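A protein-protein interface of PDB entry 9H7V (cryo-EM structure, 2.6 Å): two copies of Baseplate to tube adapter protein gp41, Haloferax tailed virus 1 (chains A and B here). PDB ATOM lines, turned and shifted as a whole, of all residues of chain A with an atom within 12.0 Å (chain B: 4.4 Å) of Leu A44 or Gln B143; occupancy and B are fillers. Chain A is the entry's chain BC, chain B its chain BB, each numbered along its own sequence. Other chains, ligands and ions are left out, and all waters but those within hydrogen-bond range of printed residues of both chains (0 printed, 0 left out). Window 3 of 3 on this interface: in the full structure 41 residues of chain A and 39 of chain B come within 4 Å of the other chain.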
ATOM      1  N   VAL A  37      10.678   5.174 -31.801  1.00  0.00           N
ATOM      2  CA  VAL A  37      11.471   3.961 -31.700  1.00  0.00           C
ATOM      3  C   VAL A  37      12.933   4.382 -31.799  1.00  0.00           C
ATOM      4  O   VAL A  37      13.311   5.098 -32.725  1.00  0.00           O
ATOM      5  CB  VAL A  37      11.090   2.940 -32.793  1.00  0.00           C
ATOM      6  CG1 VAL A  37      11.898   1.655 -32.693  1.00  0.00           C
ATOM      7  CG2 VAL A  37       9.602   2.625 -32.789  1.00  0.00           C
ATOM      8  N   ARG A  38      13.736   3.940 -30.826  1.00  0.00           N
ATOM      9  CA  ARG A  38      15.129   4.340 -30.728  1.00  0.00           C
ATOM     10  C   ARG A  38      15.934   3.618 -31.804  1.00  0.00           C
ATOM     11  O   ARG A  38      15.872   2.395 -31.919  1.00  0.00           O
ATOM     12  CB  ARG A  38      15.656   4.112 -29.307  1.00  0.00           C
ATOM     13  CG  ARG A  38      15.372   5.250 -28.335  1.00  0.00           C
ATOM     14  CD  ARG A  38      13.944   5.765 -28.300  1.00  0.00           C
ATOM     15  NE  ARG A  38      13.615   6.543 -27.116  1.00  0.00           N
ATOM     16  CZ  ARG A  38      13.392   7.854 -27.087  1.00  0.00           C
ATOM     17  NH1 ARG A  38      13.096   8.437 -25.940  1.00  0.00           N
ATOM     18  NH2 ARG A  38      13.468   8.577 -28.191  1.00  0.00           N
ATOM     19  N   LYS A  39      16.672   4.409 -32.589  1.00  0.00           N
ATOM     20  CA  LYS A  39      17.417   3.926 -33.738  1.00  0.00           C
ATOM     21  C   LYS A  39      18.680   3.202 -33.273  1.00  0.00           C
ATOM     22  O   LYS A  39      19.201   2.347 -33.987  1.00  0.00           O
ATOM     23  CB  LYS A  39      17.724   5.089 -34.687  1.00  0.00           C
ATOM     24  CG  LYS A  39      16.500   5.756 -35.304  1.00  0.00           C
ATOM     25  CD  LYS A  39      16.795   7.078 -35.979  1.00  0.00           C
ATOM     26  CE  LYS A  39      17.470   6.925 -37.326  1.00  0.00           C
ATOM     27  NZ  LYS A  39      17.930   8.226 -37.864  1.00  0.00           N
ATOM     28  N   SER A  40      19.147   3.552 -32.066  1.00  0.00           N
ATOM     29  CA  SER A  40      20.348   2.996 -31.463  1.00  0.00           C
ATOM     30  C   SER A  40      20.129   2.785 -29.964  1.00  0.00           C
ATOM     31  O   SER A  40      19.011   2.942 -29.474  1.00  0.00           O
ATOM     32  CB  SER A  40      21.530   3.885 -31.741  1.00  0.00           C
ATOM     33  OG  SER A  40      22.745   3.232 -31.407  1.00  0.00           O
ATOM     34  N   GLY A  41      21.204   2.423 -29.248  1.00  0.00           N
ATOM     35  CA  GLY A  41      21.148   2.066 -27.838  1.00  0.00           C
ATOM     36  C   GLY A  41      21.784   0.700 -27.589  1.00  0.00           C
ATOM     37  O   GLY A  41      21.948  -0.078 -28.523  1.00  0.00           O
ATOM     38  N   GLY A  42      22.106   0.407 -26.322  1.00  0.00           N
ATOM     39  CA  GLY A  42      22.926  -0.745 -25.968  1.00  0.00           C
ATOM     40  C   GLY A  42      22.139  -2.035 -25.735  1.00  0.00           C
ATOM     41  O   GLY A  42      22.698  -3.012 -25.240  1.00  0.00           O
ATOM     42  N   SER A  43      20.848  -2.028 -26.097  1.00  0.00           N
ATOM     43  CA  SER A  43      19.974  -3.187 -25.994  1.00  0.00           C
ATOM     44  C   SER A  43      19.974  -3.947 -27.318  1.00  0.00           C
ATOM     45  O   SER A  43      20.401  -3.406 -28.334  1.00  0.00           O
ATOM     46  CB  SER A  43      18.574  -2.765 -25.629  1.00  0.00           C
ATOM     47  OG  SER A  43      18.576  -1.851 -24.545  1.00  0.00           O
ATOM     48  N   LEU A  44      19.493  -5.200 -27.298  1.00  0.00           N
ATOM     49  CA  LEU A  44      19.240  -5.941 -28.526  1.00  0.00           C
ATOM     50  C   LEU A  44      18.025  -5.349 -29.238  1.00  0.00           C
ATOM     51  O   LEU A  44      18.041  -5.191 -30.457  1.00  0.00           O
ATOM     52  CB  LEU A  44      19.026  -7.428 -28.218  1.00  0.00           C
ATOM     53  CG  LEU A  44      20.252  -8.334 -28.348  1.00  0.00           C
ATOM     54  CD1 LEU A  44      19.954  -9.721 -27.802  1.00  0.00           C
ATOM     55  CD2 LEU A  44      20.725  -8.432 -29.795  1.00  0.00           C
ATOM     56  N   ASN A  45      16.988  -5.018 -28.457  1.00  0.00           N
ATOM     57  CA  ASN A  45      15.724  -4.514 -28.969  1.00  0.00           C
ATOM     58  C   ASN A  45      15.514  -3.082 -28.480  1.00  0.00           C
ATOM     59  O   ASN A  45      15.857  -2.774 -27.341  1.00  0.00           O
ATOM     60  CB  ASN A  45      14.558  -5.415 -28.554  1.00  0.00           C
ATOM     61  CG  ASN A  45      14.755  -6.874 -28.910  1.00  0.00           C
ATOM     62  OD1 ASN A  45      14.954  -7.218 -30.073  1.00  0.00           O
ATOM     63  ND2 ASN A  45      14.683  -7.743 -27.915  1.00  0.00           N
ATOM     64  N   PRO A  46      14.930  -2.172 -29.300  1.00  0.00           N
ATOM     65  CA  PRO A  46      14.840  -0.755 -28.937  1.00  0.00           C
ATOM     66  C   PRO A  46      13.898  -0.459 -27.774  1.00  0.00           C
ATOM     67  O   PRO A  46      12.960  -1.212 -27.515  1.00  0.00           O
ATOM     68  CB  PRO A  46      14.294  -0.093 -30.211  1.00  0.00           C
ATOM     69  CG  PRO A  46      13.521  -1.191 -30.899  1.00  0.00           C
ATOM     70  CD  PRO A  46      14.317  -2.446 -30.611  1.00  0.00           C
ATOM     71  N   ARG A  47      14.186   0.642 -27.076  1.00  0.00           N
ATOM     72  CA  ARG A  47      13.209   1.291 -26.223  1.00  0.00           C
ATOM     73  C   ARG A  47      12.299   2.145 -27.098  1.00  0.00           C
ATOM     74  O   ARG A  47      12.725   2.655 -28.134  1.00  0.00           O
ATOM     75  CB  ARG A  47      13.900   2.132 -25.147  1.00  0.00           C
ATOM     76  CG  ARG A  47      14.307   1.331 -23.921  1.00  0.00           C
ATOM     77  CD  ARG A  47      14.857   2.202 -22.812  1.00  0.00           C
ATOM     78  NE  ARG A  47      14.533   1.635 -21.510  1.00  0.00           N
ATOM     79  CZ  ARG A  47      15.319   0.831 -20.801  1.00  0.00           C
ATOM     80  NH1 ARG A  47      14.911   0.378 -19.629  1.00  0.00           N
ATOM     81  NH2 ARG A  47      16.509   0.485 -21.257  1.00  0.00           N
ATOM     82  N   VAL A  48      11.039   2.273 -26.665  1.00  0.00           N
ATOM     83  CA  VAL A  48      10.026   3.024 -27.388  1.00  0.00           C
ATOM     84  C   VAL A  48       9.302   3.961 -26.423  1.00  0.00           C
ATOM     85  O   VAL A  48       9.353   3.772 -25.209  1.00  0.00           O
ATOM     86  CB  VAL A  48       9.027   2.108 -28.128  1.00  0.00           C
ATOM     87  CG1 VAL A  48       9.678   1.327 -29.259  1.00  0.00           C
ATOM     88  CG2 VAL A  48       8.262   1.180 -27.193  1.00  0.00           C
ATOM     89  N   LYS B  78      20.889 -12.525 -35.647  1.00  0.00           N
ATOM     90  CA  LYS B  78      20.648 -11.343 -34.829  1.00  0.00           C
ATOM     91  C   LYS B  78      21.744 -11.125 -33.784  1.00  0.00           C
ATOM     92  O   LYS B  78      21.931  -9.997 -33.330  1.00  0.00           O
ATOM     93  CB  LYS B  78      19.254 -11.358 -34.191  1.00  0.00           C
ATOM     94  CG  LYS B  78      18.660  -9.974 -33.959  1.00  0.00           C
ATOM     95  CD  LYS B  78      17.237  -9.972 -33.449  1.00  0.00           C
ATOM     96  CE  LYS B  78      17.143 -10.140 -31.947  1.00  0.00           C
ATOM     97  NZ  LYS B  78      15.823  -9.713 -31.432  1.00  0.00           N
ATOM     98  N   THR B  79      22.457 -12.197 -33.410  1.00  0.00           N
ATOM     99  CA  THR B  79      23.451 -12.191 -32.344  1.00  0.00           C
ATOM    100  C   THR B  79      24.606 -11.250 -32.688  1.00  0.00           C
ATOM    101  O   THR B  79      25.086 -11.244 -33.820  1.00  0.00           O
ATOM    102  CB  THR B  79      23.919 -13.626 -32.048  1.00  0.00           C
ATOM    103  OG1 THR B  79      22.848 -14.295 -31.384  1.00  0.00           O
ATOM    104  CG2 THR B  79      25.162 -13.720 -31.191  1.00  0.00           C
ATOM    105  N   ASP B 141      29.208  -8.462 -26.741  1.00  0.00           N
ATOM    106  CA  ASP B 141      28.730  -9.823 -26.917  1.00  0.00           C
ATOM    107  C   ASP B 141      27.280  -9.877 -26.445  1.00  0.00           C
ATOM    108  O   ASP B 141      27.007  -9.673 -25.262  1.00  0.00           O
ATOM    109  CB  ASP B 141      29.649 -10.807 -26.179  1.00  0.00           C
ATOM    110  CG  ASP B 141      29.232 -12.270 -26.218  1.00  0.00           C
ATOM    111  OD1 ASP B 141      28.461 -12.652 -27.124  1.00  0.00           O
ATOM    112  OD2 ASP B 141      29.701 -13.027 -25.343  1.00  0.00           O
ATOM    113  N   GLN B 142      26.360 -10.132 -27.386  1.00  0.00           N
ATOM    114  CA  GLN B 142      24.935 -10.186 -27.099  1.00  0.00           C
ATOM    115  C   GLN B 142      24.313 -11.398 -27.787  1.00  0.00           C
ATOM    116  O   GLN B 142      24.062 -11.379 -28.992  1.00  0.00           O
ATOM    117  CB  GLN B 142      24.242  -8.880 -27.498  1.00  0.00           C
ATOM    118  CG  GLN B 142      24.508  -7.730 -26.537  1.00  0.00           C
ATOM    119  CD  GLN B 142      23.723  -6.476 -26.840  1.00  0.00           C
ATOM    120  OE1 GLN B 142      23.278  -6.243 -27.962  1.00  0.00           O
ATOM    121  NE2 GLN B 142      23.554  -5.644 -25.826  1.00  0.00           N
ATOM    122  N   GLN B 143      24.077 -12.445 -26.990  1.00  0.00           N
ATOM    123  CA  GLN B 143      23.408 -13.659 -27.424  1.00  0.00           C
ATOM    124  C   GLN B 143      21.916 -13.370 -27.573  1.00  0.00           C
ATOM    125  O   GLN B 143      21.253 -13.017 -26.600  1.00  0.00           O
ATOM    126  CB  GLN B 143      23.679 -14.775 -26.409  1.00  0.00           C
ATOM    127  CG  GLN B 143      23.088 -16.129 -26.784  1.00  0.00           C
ATOM    128  CD  GLN B 143      23.614 -16.664 -28.094  1.00  0.00           C
ATOM    129  OE1 GLN B 143      24.818 -16.689 -28.344  1.00  0.00           O
ATOM    130  NE2 GLN B 143      22.704 -17.101 -28.949  1.00  0.00           N
ATOM    131  N   ALA B 144      21.409 -13.509 -28.805  1.00  0.00           N
ATOM    132  CA  ALA B 144      19.989 -13.376 -29.086  1.00  0.00           C
ATOM    133  C   ALA B 144      19.281 -14.688 -28.761  1.00  0.00           C
ATOM    134  O   ALA B 144      19.811 -15.764 -29.037  1.00  0.00           O
ATOM    135  CB  ALA B 144      19.783 -12.977 -30.526  1.00  0.00           C
ATOM    136  N   THR B 145      18.088 -14.584 -28.156  1.00  0.00           N
ATOM    137  CA  THR B 145      17.227 -15.738 -27.932  1.00  0.00           C
ATOM    138  C   THR B 145      15.805 -15.430 -28.391  1.00  0.00           C
ATOM    139  O   THR B 145      15.210 -14.435 -27.977  1.00  0.00           O
ATOM    140  CB  THR B 145      17.223 -16.214 -26.471  1.00  0.00           C
ATOM    141  OG1 THR B 145      16.783 -15.151 -25.627  1.00  0.00           O
ATOM    142  CG2 THR B 145      18.559 -16.746 -25.997  1.00  0.00           C
ATOM    143  N   VAL B 201      21.188  -1.826 -30.959  1.00  0.00           N
ATOM    144  CA  VAL B 201      19.810  -2.143 -31.306  1.00  0.00           C
ATOM    145  C   VAL B 201      19.735  -2.804 -32.683  1.00  0.00           C
ATOM    146  O   VAL B 201      20.405  -2.380 -33.624  1.00  0.00           O
ATOM    147  CB  VAL B 201      18.918  -0.888 -31.180  1.00  0.00           C
ATOM    148  CG1 VAL B 201      17.630  -0.966 -31.988  1.00  0.00           C
ATOM    149  CG2 VAL B 201      18.611  -0.559 -29.727  1.00  0.00           C
ATOM    150  N   THR B 202      18.906  -3.853 -32.760  1.00  0.00           N
ATOM    151  CA  THR B 202      18.696  -4.652 -33.957  1.00  0.00           C
ATOM    152  C   THR B 202      17.263  -4.474 -34.453  1.00  0.00           C
ATOM    153  O   THR B 202      16.441  -3.845 -33.788  1.00  0.00           O
ATOM    154  CB  THR B 202      18.989  -6.134 -33.687  1.00  0.00           C
ATOM    155  OG1 THR B 202      18.068  -6.619 -32.708  1.00  0.00           O
ATOM    156  CG2 THR B 202      20.406  -6.390 -33.225  1.00  0.00           C
ATOM    157  N   ASN B 284      14.847  -7.690 -22.903  1.00  0.00           N
ATOM    158  CA  ASN B 284      15.868  -8.731 -22.929  1.00  0.00           C
ATOM    159  C   ASN B 284      16.864  -8.554 -21.779  1.00  0.00           C
ATOM    160  O   ASN B 284      17.996  -9.034 -21.853  1.00  0.00           O
ATOM    161  CB  ASN B 284      16.544  -8.784 -24.306  1.00  0.00           C
ATOM    162  CG  ASN B 284      16.930 -10.177 -24.763  1.00  0.00           C
ATOM    163  OD1 ASN B 284      16.608 -10.577 -25.879  1.00  0.00           O
ATOM    164  ND2 ASN B 284      17.633 -10.921 -23.922  1.00  0.00           N
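N of Val B201 lies within hydrogen-bond range of O of Gly A41 (3.1 Å). The side-chain amide nitrogen of Gln B142 is in hydrogen-bond range of the backbone carbonyl oxygen of Gly A42 (2.8 Å). The backbone NH (N) of Val B201 lies within hydrogen-bond range of the backbone carbonyl oxygen (O) of Ser A43 (3.2 Å). The side-chain hydroxyl of Thr B202 is in hydrogen-bond range of the backbone carbonyl oxygen of Leu A44 (2.7 Å). OD1 of Asn A45 lies within hydrogen-bond range of NZ of Lys B78 (3.0 Å).
N of Ala B144 is in hydrogen-bond range of OG1 of Thr B79. N of Arg A38 sits at hydrogen-bond distance from O of Arg A47, 3.1 Å away.
Among the printed residues, merely in contact across the chains: Arg A38 with Val B201 (3.8 Å), Ser A40 with Val B201 (3.5 Å), Leu A44 with Gln B142 (3.7 Å), Leu A44 with Gln B143 (3.7 Å), Leu A44 with Ala B144 (3.9 Å), Leu A44 with Val B201 (3.6 Å), Leu A44 with Asn B284 (3.95 Å), Asn A45 with Asn B284 (3.99 Å) and Pro A46 with Val B201 (3.9 Å).
Val A37 touches none of the printed residues of chain B. Of chain B, only Gln B142, Gln B143, Ala B144, Val B201, Thr B202 and Asn B284 come within 4 Å of Leu A44. Of the printed residues of chain B, Asn A45 touches Lys B78 and Asn B284. Of the printed residues of chain B, Pro A46 touches Val B201. Lys B78 touches just one residue of chain A: Asn A45. Gln B142 touches two residues of chain A. Gln B143 touches one residue of chain A. Of chain A, only Leu A44 comes within 4 Å of Ala B144. No residue of chain A comes within 4 Å of Thr B145. Of chain A, only Arg A38, Ser A40, Gly A41, Ser A43, Leu A44 and Pro A46 come within 4 Å of Val B201. Thr B202 touches one residue of chain A. Of the printed residues of chain A, Asn B284 touches Leu A44 and Asn A45. The nearest residue of chain B that does not touch Leu A44 is Lys B78 (4.05 Å). The nearest residue of chain A that does not touch Gln B143 is Asn A45 (8.5 Å).
Of the 10 printed residues of chain B, 7 touch a printed residue of chain A. Printed residues of chain B that touch a printed residue of chain A: Lys B78, Gln B142, Gln B143, Ala B144, Val B201, Thr B202 and Asn B284. Hydrophobic or aromatic side chains of chain B within 4 Å of the printed part of chain A: Val B201. Printed residues of chain A that touch a printed residue of chain B: Arg A38, Ser A40, Gly A41, Gly A42, Ser A43, Leu A44, Asn A45 and Pro A46. Among the printed residues, 14 pairs touch across the chains. Among the printed residues, no Asp or Glu carboxylate lies within 4 Å of a Lys or Arg side-chain nitrogen of the other chain.
No position is printed for both chains.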
